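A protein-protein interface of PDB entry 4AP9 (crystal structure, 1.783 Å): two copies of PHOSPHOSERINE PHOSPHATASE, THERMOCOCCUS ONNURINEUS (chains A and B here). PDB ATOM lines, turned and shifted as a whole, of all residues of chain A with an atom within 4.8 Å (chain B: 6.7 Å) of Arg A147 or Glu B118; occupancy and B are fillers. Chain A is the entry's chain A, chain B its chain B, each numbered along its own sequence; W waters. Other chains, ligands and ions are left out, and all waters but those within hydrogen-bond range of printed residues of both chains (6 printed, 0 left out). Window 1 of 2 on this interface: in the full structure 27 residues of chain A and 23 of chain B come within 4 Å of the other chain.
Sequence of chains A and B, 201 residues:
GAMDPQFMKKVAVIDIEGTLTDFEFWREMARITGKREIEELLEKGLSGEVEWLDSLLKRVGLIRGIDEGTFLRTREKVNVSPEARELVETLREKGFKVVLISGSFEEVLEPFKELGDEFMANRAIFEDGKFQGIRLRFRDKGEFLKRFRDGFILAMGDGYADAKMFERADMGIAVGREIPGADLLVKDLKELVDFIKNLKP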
ATOM      1  N   MET A 120      20.631 -22.573  30.812  1.00  0.00           N
ATOM      2  CA  MET A 120      21.685 -22.384  29.818  1.00  0.00           C
ATOM      3  C   MET A 120      21.624 -21.018  29.149  1.00  0.00           C
ATOM      4  O   MET A 120      20.591 -20.632  28.607  1.00  0.00           O
ATOM      5  CB  MET A 120      21.602 -23.435  28.712  1.00  0.00           C
ATOM      6  CG  MET A 120      22.469 -23.105  27.488  1.00  0.00           C
ATOM      7  SD  MET A 120      24.374 -23.365  27.834  1.00  0.00           S
ATOM      8  CE  MET A 120      24.147 -24.982  28.837  1.00  0.00           C
ATOM      9  N   ARG A 137      27.887 -20.529  23.630  1.00  0.00           N
ATOM     10  CA  ARG A 137      27.862 -21.851  24.250  1.00  0.00           C
ATOM     11  C   ARG A 137      26.903 -22.810  23.556  1.00  0.00           C
ATOM     12  O   ARG A 137      26.835 -23.999  23.891  1.00  0.00           O
ATOM     13  CB  ARG A 137      27.548 -21.694  25.732  1.00  0.00           C
ATOM     14  CG  ARG A 137      28.558 -20.766  26.410  1.00  0.00           C
ATOM     15  CD  ARG A 137      28.394 -20.709  27.913  1.00  0.00           C
ATOM     16  NE  ARG A 137      28.609 -22.017  28.524  1.00  0.00           N
ATOM     17  CZ  ARG A 137      27.743 -22.598  29.347  1.00  0.00           C
ATOM     18  NH1 ARG A 137      26.614 -21.983  29.661  1.00  0.00           N
ATOM     19  NH2 ARG A 137      28.009 -23.787  29.864  1.00  0.00           N
ATOM     20  N   GLU A 143      19.358 -25.403  17.813  1.00  0.00           N
ATOM     21  CA  GLU A 143      20.425 -26.391  17.943  1.00  0.00           C
ATOM     22  C   GLU A 143      20.496 -26.871  19.377  1.00  0.00           C
ATOM     23  O   GLU A 143      20.683 -28.063  19.637  1.00  0.00           O
ATOM     24  CB  GLU A 143      21.786 -25.812  17.535  1.00  0.00           C
ATOM     25  CG  GLU A 143      22.010 -25.737  16.050  1.00  0.00           C
ATOM     26  CD  GLU A 143      21.779 -27.068  15.362  1.00  0.00           C
ATOM     27  OE1 GLU A 143      22.522 -28.031  15.639  1.00  0.00           O
ATOM     28  OE2 GLU A 143      20.852 -27.134  14.542  1.00  0.00           O
ATOM     29  N   PHE A 144      20.329 -25.942  20.315  1.00  0.00           N
ATOM     30  CA  PHE A 144      20.381 -26.307  21.724  1.00  0.00           C
ATOM     31  C   PHE A 144      19.313 -27.342  22.085  1.00  0.00           C
ATOM     32  O   PHE A 144      19.566 -28.254  22.870  1.00  0.00           O
ATOM     33  CB  PHE A 144      20.229 -25.089  22.636  1.00  0.00           C
ATOM     34  CG  PHE A 144      20.222 -25.442  24.089  1.00  0.00           C
ATOM     35  CD1 PHE A 144      21.382 -25.875  24.708  1.00  0.00           C
ATOM     36  CD2 PHE A 144      19.059 -25.364  24.830  1.00  0.00           C
ATOM     37  CE1 PHE A 144      21.372 -26.225  26.053  1.00  0.00           C
ATOM     38  CE2 PHE A 144      19.052 -25.707  26.179  1.00  0.00           C
ATOM     39  CZ  PHE A 144      20.215 -26.133  26.777  1.00  0.00           C
ATOM     40  N   LEU A 145      18.121 -27.190  21.524  1.00  0.00           N
ATOM     41  CA  LEU A 145      17.018 -28.118  21.803  1.00  0.00           C
ATOM     42  C   LEU A 145      17.296 -29.577  21.425  1.00  0.00           C
ATOM     43  O   LEU A 145      16.636 -30.479  21.941  1.00  0.00           O
ATOM     44  CB  LEU A 145      15.716 -27.646  21.151  1.00  0.00           C
ATOM     45  CG  LEU A 145      14.691 -26.948  22.055  1.00  0.00           C
ATOM     46  CD1 LEU A 145      15.282 -25.725  22.730  1.00  0.00           C
ATOM     47  CD2 LEU A 145      13.424 -26.581  21.280  1.00  0.00           C
ATOM     48  N   LYS A 146      18.250 -29.800  20.526  1.00  0.00           N
ATOM     49  CA  LYS A 146      18.667 -31.159  20.166  1.00  0.00           C
ATOM     50  C   LYS A 146      19.122 -31.953  21.387  1.00  0.00           C
ATOM     51  O   LYS A 146      19.160 -33.180  21.364  1.00  0.00           O
ATOM     52  CB  LYS A 146      19.790 -31.126  19.128  1.00  0.00           C
ATOM     53  CG  LYS A 146      19.378 -30.650  17.748  1.00  0.00           C
ATOM     54  CD  LYS A 146      20.570 -30.695  16.804  1.00  0.00           C
ATOM     55  CE  LYS A 146      20.178 -30.358  15.377  1.00  0.00           C
ATOM     56  NZ  LYS A 146      21.363 -30.326  14.457  1.00  0.00           N
ATOM     57  N   ARG A 147      19.483 -31.235  22.448  1.00  0.00           N
ATOM     58  CA  ARG A 147      19.856 -31.844  23.720  1.00  0.00           C
ATOM     59  C   ARG A 147      18.728 -32.714  24.293  1.00  0.00           C
ATOM     60  O   ARG A 147      18.966 -33.670  25.037  1.00  0.00           O
ATOM     61  CB  ARG A 147      20.169 -30.700  24.681  1.00  0.00           C
ATOM     62  CG  ARG A 147      20.835 -31.088  25.955  1.00  0.00           C
ATOM     63  CD  ARG A 147      21.447 -29.845  26.586  1.00  0.00           C
ATOM     64  NE  ARG A 147      22.720 -29.483  25.967  1.00  0.00           N
ATOM     65  CZ  ARG A 147      23.762 -29.029  26.661  1.00  0.00           C
ATOM     66  NH1 ARG A 147      23.655 -28.880  27.975  1.00  0.00           N
ATOM     67  NH2 ARG A 147      24.901 -28.715  26.050  1.00  0.00           N
ATOM     68  N   PHE A 148      17.496 -32.370  23.928  1.00  0.00           N
ATOM     69  CA  PHE A 148      16.314 -33.037  24.443  1.00  0.00           C
ATOM     70  C   PHE A 148      15.559 -33.771  23.336  1.00  0.00           C
ATOM     71  O   PHE A 148      14.345 -33.915  23.391  1.00  0.00           O
ATOM     72  CB  PHE A 148      15.429 -31.992  25.136  1.00  0.00           C
ATOM     73  CG  PHE A 148      16.197 -31.144  26.105  1.00  0.00           C
ATOM     74  CD1 PHE A 148      16.573 -31.655  27.333  1.00  0.00           C
ATOM     75  CD2 PHE A 148      16.588 -29.862  25.767  1.00  0.00           C
ATOM     76  CE1 PHE A 148      17.308 -30.891  28.225  1.00  0.00           C
ATOM     77  CE2 PHE A 148      17.331 -29.097  26.647  1.00  0.00           C
ATOM     78  CZ  PHE A 148      17.689 -29.603  27.870  1.00  0.00           C
ATOM     79  N   ARG A 149      16.296 -34.256  22.344  1.00  0.00           N
ATOM     80  CA  ARG A 149      15.693 -34.870  21.169  1.00  0.00           C
ATOM     81  C   ARG A 149      15.044 -36.214  21.473  1.00  0.00           C
ATOM     82  O   ARG A 149      14.197 -36.667  20.719  1.00  0.00           O
ATOM     83  CB  ARG A 149      16.731 -35.038  20.058  1.00  0.00           C
ATOM     84  CG  ARG A 149      17.867 -35.992  20.417  1.00  0.00           C
ATOM     85  CD  ARG A 149      19.001 -35.945  19.393  1.00  0.00           C
ATOM     86  NE  ARG A 149      18.646 -36.554  18.112  1.00  0.00           N
ATOM     87  CZ  ARG A 149      18.927 -37.811  17.780  1.00  0.00           C
ATOM     88  NH1 ARG A 149      19.557 -38.606  18.639  1.00  0.00           N
ATOM     89  NH2 ARG A 149      18.573 -38.279  16.591  1.00  0.00           N
ATOM     90  N   GLN B   6      32.811 -21.796  22.104  1.00  0.00           N
ATOM     91  CA  GLN B   6      32.795 -22.946  22.993  1.00  0.00           C
ATOM     92  C   GLN B   6      31.949 -24.091  22.425  1.00  0.00           C
ATOM     93  O   GLN B   6      32.305 -25.268  22.557  1.00  0.00           O
ATOM     94  CB  GLN B   6      32.287 -22.512  24.375  1.00  0.00           C
ATOM     95  CG  GLN B   6      32.247 -23.619  25.415  1.00  0.00           C
ATOM     96  CD  GLN B   6      31.587 -23.165  26.708  1.00  0.00           C
ATOM     97  OE1 GLN B   6      32.027 -22.212  27.346  1.00  0.00           O
ATOM     98  NE2 GLN B   6      30.521 -23.846  27.094  1.00  0.00           N
ATOM     99  N   ARG B  92      41.128 -26.954  29.477  1.00  0.00           N
ATOM    100  CA  ARG B  92      40.687 -25.745  28.777  1.00  0.00           C
ATOM    101  C   ARG B  92      41.795 -25.174  27.918  1.00  0.00           C
ATOM    102  O   ARG B  92      41.554 -24.730  26.797  1.00  0.00           O
ATOM    103  CB  ARG B  92      40.201 -24.676  29.752  1.00  0.00           C
ATOM    104  CG  ARG B  92      38.816 -24.926  30.285  1.00  0.00           C
ATOM    105  CD  ARG B  92      38.128 -23.623  30.667  1.00  0.00           C
ATOM    106  NE  ARG B  92      36.943 -23.905  31.458  1.00  0.00           N
ATOM    107  CZ  ARG B  92      36.954 -24.025  32.780  1.00  0.00           C
ATOM    108  NH1 ARG B  92      38.089 -23.874  33.452  1.00  0.00           N
ATOM    109  NH2 ARG B  92      35.830 -24.294  33.431  1.00  0.00           N
ATOM    110  N   LYS B  97      36.119 -28.164  25.922  1.00  0.00           N
ATOM    111  CA  LYS B  97      35.011 -27.751  26.767  1.00  0.00           C
ATOM    112  C   LYS B  97      34.895 -28.834  27.840  1.00  0.00           C
ATOM    113  O   LYS B  97      34.892 -30.017  27.508  1.00  0.00           O
ATOM    114  CB  LYS B  97      33.748 -27.710  25.921  1.00  0.00           C
ATOM    115  CG  LYS B  97      32.469 -27.442  26.657  1.00  0.00           C
ATOM    116  CD  LYS B  97      31.305 -27.504  25.693  1.00  0.00           C
ATOM    117  CE  LYS B  97      30.060 -27.959  26.414  1.00  0.00           C
ATOM    118  NZ  LYS B  97      28.807 -27.609  25.706  1.00  0.00           N
ATOM    119  N   VAL B  98      34.822 -28.447  29.113  1.00  0.00           N
ATOM    120  CA  VAL B  98      34.878 -29.432  30.199  1.00  0.00           C
ATOM    121  C   VAL B  98      33.509 -29.673  30.836  1.00  0.00           C
ATOM    122  O   VAL B  98      32.837 -28.734  31.259  1.00  0.00           O
ATOM    123  CB  VAL B  98      35.913 -29.019  31.277  1.00  0.00           C
ATOM    124  CG1 VAL B  98      35.982 -30.054  32.397  1.00  0.00           C
ATOM    125  CG2 VAL B  98      37.287 -28.843  30.646  1.00  0.00           C
ATOM    126  N   VAL B  99      33.105 -30.935  30.925  1.00  0.00           N
ATOM    127  CA  VAL B  99      31.819 -31.290  31.507  1.00  0.00           C
ATOM    128  C   VAL B  99      32.053 -32.268  32.646  1.00  0.00           C
ATOM    129  O   VAL B  99      32.651 -33.317  32.436  1.00  0.00           O
ATOM    130  CB  VAL B  99      30.907 -31.962  30.464  1.00  0.00           C
ATOM    131  CG1 VAL B  99      29.581 -32.387  31.088  1.00  0.00           C
ATOM    132  CG2 VAL B  99      30.669 -31.011  29.285  1.00  0.00           C
ATOM    133  N   LEU B 100      31.595 -31.923  33.846  1.00  0.00           N
ATOM    134  CA  LEU B 100      31.740 -32.814  34.992  1.00  0.00           C
ATOM    135  C   LEU B 100      30.419 -33.524  35.235  1.00  0.00           C
ATOM    136  O   LEU B 100      29.363 -32.885  35.249  1.00  0.00           O
ATOM    137  CB  LEU B 100      32.170 -32.012  36.233  1.00  0.00           C
ATOM    138  CG  LEU B 100      33.424 -31.128  36.088  1.00  0.00           C
ATOM    139  CD1 LEU B 100      33.760 -30.463  37.434  1.00  0.00           C
ATOM    140  CD2 LEU B 100      34.655 -31.891  35.555  1.00  0.00           C
ATOM    141  N   ILE B 101      30.469 -34.841  35.432  1.00  0.00           N
ATOM    142  CA  ILE B 101      29.252 -35.632  35.657  1.00  0.00           C
ATOM    143  C   ILE B 101      29.447 -36.540  36.863  1.00  0.00           C
ATOM    144  O   ILE B 101      30.580 -36.954  37.170  1.00  0.00           O
ATOM    145  CB  ILE B 101      28.912 -36.519  34.442  1.00  0.00           C
ATOM    146  CG1 ILE B 101      27.641 -37.331  34.672  1.00  0.00           C
ATOM    147  CG2 ILE B 101      30.045 -37.498  34.142  1.00  0.00           C
ATOM    148  CD1 ILE B 101      26.375 -36.623  34.300  1.00  0.00           C
ATOM    149  N   PHE B 112      32.176 -28.659  43.203  1.00  0.00           N
ATOM    150  CA  PHE B 112      32.624 -28.839  41.825  1.00  0.00           C
ATOM    151  C   PHE B 112      31.725 -28.130  40.819  1.00  0.00           C
ATOM    152  O   PHE B 112      32.002 -28.131  39.617  1.00  0.00           O
ATOM    153  CB  PHE B 112      32.637 -30.332  41.490  1.00  0.00           C
ATOM    154  CG  PHE B 112      33.727 -31.090  42.175  1.00  0.00           C
ATOM    155  CD1 PHE B 112      35.022 -31.068  41.673  1.00  0.00           C
ATOM    156  CD2 PHE B 112      33.465 -31.825  43.314  1.00  0.00           C
ATOM    157  CE1 PHE B 112      36.037 -31.770  42.295  1.00  0.00           C
ATOM    158  CE2 PHE B 112      34.479 -32.537  43.944  1.00  0.00           C
ATOM    159  CZ  PHE B 112      35.765 -32.498  43.438  1.00  0.00           C
ATOM    160  N   LYS B 113      30.657 -27.521  41.316  1.00  0.00           N
ATOM    161  CA  LYS B 113      29.562 -27.056  40.470  1.00  0.00           C
ATOM    162  C   LYS B 113      29.993 -26.080  39.378  1.00  0.00           C
ATOM    163  O   LYS B 113      29.473 -26.130  38.263  1.00  0.00           O
ATOM    164  CB  LYS B 113      28.478 -26.417  41.347  1.00  0.00           C
ATOM    165  CG  LYS B 113      27.180 -26.036  40.649  1.00  0.00           C
ATOM    166  CD  LYS B 113      26.241 -25.320  41.632  1.00  0.00           C
ATOM    167  CE  LYS B 113      25.250 -26.279  42.298  1.00  0.00           C
ATOM    168  NZ  LYS B 113      24.441 -25.635  43.383  1.00  0.00           N
ATOM    169  N   LEU B 115      33.327 -25.613  38.481  1.00  0.00           N
ATOM    170  CA  LEU B 115      34.704 -25.908  38.093  1.00  0.00           C
ATOM    171  C   LEU B 115      34.856 -26.066  36.586  1.00  0.00           C
ATOM    172  O   LEU B 115      35.724 -25.434  35.977  1.00  0.00           O
ATOM    173  CB  LEU B 115      35.199 -27.171  38.795  1.00  0.00           C
ATOM    174  CG  LEU B 115      36.633 -27.584  38.476  1.00  0.00           C
ATOM    175  CD1 LEU B 115      37.595 -26.448  38.798  1.00  0.00           C
ATOM    176  CD2 LEU B 115      36.980 -28.834  39.266  1.00  0.00           C
ATOM    177  N   GLY B 116      34.015 -26.914  35.994  1.00  0.00           N
ATOM    178  CA  GLY B 116      34.026 -27.129  34.559  1.00  0.00           C
ATOM    179  C   GLY B 116      33.083 -26.161  33.865  1.00  0.00           C
ATOM    180  O   GLY B 116      32.559 -25.246  34.488  1.00  0.00           O
ATOM    181  N   ASP B 117      32.863 -26.369  32.573  1.00  0.00           N
ATOM    182  CA  ASP B 117      31.960 -25.517  31.797  1.00  0.00           C
ATOM    183  C   ASP B 117      30.510 -25.951  31.939  1.00  0.00           C
ATOM    184  O   ASP B 117      29.597 -25.135  31.832  1.00  0.00           O
ATOM    185  CB  ASP B 117      32.377 -25.527  30.327  1.00  0.00           C
ATOM    186  CG  ASP B 117      33.768 -24.987  30.134  1.00  0.00           C
ATOM    187  OD1 ASP B 117      34.016 -23.857  30.594  1.00  0.00           O
ATOM    188  OD2 ASP B 117      34.612 -25.689  29.549  1.00  0.00           O
ATOM    189  N   GLU B 118      30.304 -27.245  32.160  1.00  0.00           N
ATOM    190  CA  GLU B 118      28.987 -27.748  32.518  1.00  0.00           C
ATOM    191  C   GLU B 118      29.110 -28.768  33.637  1.00  0.00           C
ATOM    192  O   GLU B 118      30.153 -29.428  33.771  1.00  0.00           O
ATOM    193  CB  GLU B 118      28.300 -28.407  31.322  1.00  0.00           C
ATOM    194  CG  GLU B 118      28.044 -27.477  30.150  1.00  0.00           C
ATOM    195  CD  GLU B 118      27.041 -28.076  29.164  1.00  0.00           C
ATOM    196  OE1 GLU B 118      25.975 -28.564  29.597  1.00  0.00           O
ATOM    197  OE2 GLU B 118      27.325 -28.060  27.953  1.00  0.00           O
ATOM    198  N   PHE B 119      28.038 -28.898  34.418  1.00  0.00           N
ATOM    199  CA  PHE B 119      28.018 -29.777  35.586  1.00  0.00           C
ATOM    200  C   PHE B 119      26.683 -30.488  35.627  1.00  0.00           C
ATOM    201  O   PHE B 119      25.640 -29.869  35.415  1.00  0.00           O
ATOM    202  CB  PHE B 119      28.228 -28.949  36.861  1.00  0.00           C
ATOM    203  CG  PHE B 119      28.108 -29.735  38.140  1.00  0.00           C
ATOM    204  CD1 PHE B 119      29.149 -30.536  38.582  1.00  0.00           C
ATOM    205  CD2 PHE B 119      26.976 -29.628  38.926  1.00  0.00           C
ATOM    206  CE1 PHE B 119      29.050 -31.239  39.776  1.00  0.00           C
ATOM    207  CE2 PHE B 119      26.868 -30.329  40.115  1.00  0.00           C
ATOM    208  CZ  PHE B 119      27.902 -31.140  40.538  1.00  0.00           C
ATOM    209  N   MET B 120      26.706 -31.793  35.875  1.00  0.00           N
ATOM    210  CA  MET B 120      25.463 -32.555  35.977  1.00  0.00           C
ATOM    211  C   MET B 120      25.598 -33.699  36.971  1.00  0.00           C
ATOM    212  O   MET B 120      26.505 -34.525  36.861  1.00  0.00           O
ATOM    213  CB  MET B 120      25.068 -33.119  34.610  1.00  0.00           C
ATOM    214  CG  MET B 120      24.036 -34.233  34.672  1.00  0.00           C
ATOM    215  SD  MET B 120      22.274 -33.522  35.117  1.00  0.00           S
ATOM    216  CE  MET B 120      22.338 -32.011  33.871  1.00  0.00           C
ATOM    217  N   PHE B 144      23.821 -39.900  28.984  1.00  0.00           N
ATOM    218  CA  PHE B 144      24.099 -38.492  29.190  1.00  0.00           C
ATOM    219  C   PHE B 144      25.048 -37.960  28.108  1.00  0.00           C
ATOM    220  O   PHE B 144      24.901 -36.831  27.632  1.00  0.00           O
ATOM    221  CB  PHE B 144      24.674 -38.252  30.590  1.00  0.00           C
ATOM    222  CG  PHE B 144      25.199 -36.864  30.788  1.00  0.00           C
ATOM    223  CD1 PHE B 144      24.329 -35.798  30.932  1.00  0.00           C
ATOM    224  CD2 PHE B 144      26.570 -36.627  30.813  1.00  0.00           C
ATOM    225  CE1 PHE B 144      24.814 -34.506  31.100  1.00  0.00           C
ATOM    226  CE2 PHE B 144      27.057 -35.342  31.003  1.00  0.00           C
ATOM    227  CZ  PHE B 144      26.167 -34.287  31.140  1.00  0.00           C
ATOM    228  N   LYS B 146      25.109 -38.507  25.117  1.00  0.00           N
ATOM    229  CA  LYS B 146      24.387 -38.224  23.876  1.00  0.00           C
ATOM    230  C   LYS B 146      24.156 -36.732  23.694  1.00  0.00           C
ATOM    231  O   LYS B 146      23.951 -36.265  22.578  1.00  0.00           O
ATOM    232  CB  LYS B 146      23.040 -38.952  23.842  1.00  0.00           C
ATOM    233  CG  LYS B 146      23.143 -40.454  23.641  1.00  0.00           C
ATOM    234  CD  LYS B 146      21.760 -41.062  23.555  1.00  0.00           C
ATOM    235  CE  LYS B 146      21.820 -42.551  23.280  1.00  0.00           C
ATOM    236  NZ  LYS B 146      20.442 -43.112  23.151  1.00  0.00           N
ATOM    237  N   ARG B 147      24.176 -35.992  24.798  1.00  0.00           N
ATOM    238  CA  ARG B 147      24.072 -34.532  24.735  1.00  0.00           C
ATOM    239  C   ARG B 147      25.141 -33.918  23.847  1.00  0.00           C
ATOM    240  O   ARG B 147      24.966 -32.807  23.341  1.00  0.00           O
ATOM    241  CB  ARG B 147      24.198 -33.915  26.131  1.00  0.00           C
ATOM    242  CG  ARG B 147      23.089 -34.299  27.055  1.00  0.00           C
ATOM    243  CD  ARG B 147      23.021 -33.362  28.241  1.00  0.00           C
ATOM    244  NE  ARG B 147      21.741 -33.547  28.895  1.00  0.00           N
ATOM    245  CZ  ARG B 147      21.163 -32.654  29.679  1.00  0.00           C
ATOM    246  NH1 ARG B 147      21.770 -31.501  29.946  1.00  0.00           N
ATOM    247  NH2 ARG B 147      19.981 -32.928  30.204  1.00  0.00           N
ATOM    248  N   PHE B 148      26.250 -34.640  23.674  1.00  0.00           N
ATOM    249  CA  PHE B 148      27.422 -34.120  22.974  1.00  0.00           C
ATOM    250  C   PHE B 148      27.713 -34.942  21.723  1.00  0.00           C
ATOM    251  O   PHE B 148      28.848 -35.003  21.259  1.00  0.00           O
ATOM    252  CB  PHE B 148      28.620 -34.100  23.933  1.00  0.00           C
ATOM    253  CG  PHE B 148      28.283 -33.496  25.261  1.00  0.00           C
ATOM    254  CD1 PHE B 148      28.072 -32.131  25.376  1.00  0.00           C
ATOM    255  CD2 PHE B 148      28.102 -34.294  26.383  1.00  0.00           C
ATOM    256  CE1 PHE B 148      27.714 -31.569  26.597  1.00  0.00           C
ATOM    257  CE2 PHE B 148      27.745 -33.729  27.604  1.00  0.00           C
ATOM    258  CZ  PHE B 148      27.567 -32.369  27.710  1.00  0.00           C
HETATM  259  O   HOH W   1      21.206 -35.439  22.143  1.00  0.00           O
HETATM  260  O   HOH W   2      26.299 -24.820  32.093  1.00  0.00           O
HETATM  261  O   HOH W   3      18.698 -34.554  27.918  1.00  0.00           O
HETATM  262  O   HOH W   4      20.864 -35.700  24.654  1.00  0.00           O
HETATM  263  O   HOH W   5      29.146 -25.063  25.027  1.00  0.00           O
HETATM  264  O   HOH W   6      25.827 -30.024  23.518  1.00  0.00           O
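The side-chain amide nitrogen (NE2) of Gln B6 lies close to the guanidinium group (NE) of Arg A137. The guanidinium group (NH2) of Arg A137 is in hydrogen-bond range of the backbone carbonyl oxygen (O) of Asp B117 (2.9 Å). NH1 of Arg A147 lies within salt-bridge range of OE1 of Glu B118, at 2.8 Å.
OD1 of Asp B117 lies within salt-bridge range of NE of Arg B92 (3.1 Å). The side-chain sulfur (SD) of Met A120 lies within hydrogen-bond range of the guanidinium group (NH1) of Arg A137, 3.2 Å away. The backbone carbonyl oxygen (O) of Val B98 is in hydrogen-bond range of the backbone NH (N) of Glu B118 (3.1 Å). N of Asp B117 is in hydrogen-bond range of O of Val B98 (2.7 Å). The side-chain carboxylate (OE2) of Glu B118 lies within salt-bridge range of the side-chain amino group (NZ) of Lys B97 (2.7 Å). The backbone NH (N) of Leu B100 lies within hydrogen-bond range of the backbone carbonyl oxygen (O) of Glu B118, at 2.9 Å.
Among the printed residues, pairs that only touch across the chains: Arg A137 with Glu B118 (3.7 Å), Arg A147 with Arg B147 (3.8 Å) and Phe A148 with Arg B147 (3.9 Å).
Arg A147 touches two residues of chain B. Glu B118 touches just these residues of chain A: Arg A137 and Arg A147. Of the printed residues of chain A, Asp B117 touches Arg A137 (2.9 Å). Of the printed residues of chain B, Phe A148 touches Arg B147 (3.9 Å). Printed residues of chain A within 4 Å of Gln B6: Arg A137. Of the printed residues of chain B, Arg A137 touches Gln B6, Asp B117 and Glu B118. Printed residues of chain A within 4 Å of Arg B147: Arg A147 and Phe A148. Lys B113 touches none of the printed residues of chain A. Arg A149 touches none of the printed residues of chain B. The nearest printed residue of chain B that does not touch Arg A147 is Phe B148 (4.04 Å). The nearest printed residue of chain B that does not touch Phe A148 is Met B120 (7.6 Å).
Of the 19 printed residues of chain B, 4 touch a printed residue of chain A. Along chain B the printed residues that touch a printed residue of chain A span positions 6 to 147. Of the 9 printed residues of chain A, 3 touch a printed residue of chain B. Hydrophobic or aromatic side chains of chain A within 4 Å of the printed part of chain B: Phe A148. Along chain A the printed residues that touch a printed residue of chain B span positions 137 to 148. Among the printed residues, 6 pairs touch across the chains.
Arg B147 touches its own counterpart, Arg A147. Phe A148 touches Arg B147, but with the chains exchanged Arg A147 does not touch Phe B148 (4.04 Å). 5 positions are printed for both chains. Of the 6 pairs that touch across the chains among the printed residues, 1 has its exchanged pair printed and touching as well.
Water W5 lies within hydrogen-bond range of the side-chain amino group (NZ) of Lys B97 (2.7 Å), the side-chain amide nitrogen (NE2) of Gln B6 (2.8 Å) and the backbone carbonyl oxygen (O) of Arg A137 (2.8 Å). Water W4 lies within hydrogen-bond range of the backbone carbonyl oxygen of Arg A147 (2.8 Å) and the backbone NH of Arg B147 (3.3 Å). Water W1 bridges the backbone carbonyl oxygen of Lys B146 (2.9 Å) and the backbone carbonyl oxygen of Lys A146 (3.1 Å). Water W6 bridges O of Arg B147 (2.9 Å) and NH2 of Arg A147 (3.0 Å). Water W2 lies within hydrogen-bond range of the guanidinium group of Arg A137 and the backbone carbonyl oxygen of Asp B117. Water W3 lies within hydrogen-bond range of the backbone carbonyl oxygen (O) of Arg A147 (3.0 Å) and the guanidinium group (NH2) of Arg B147 (3.1 Å).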
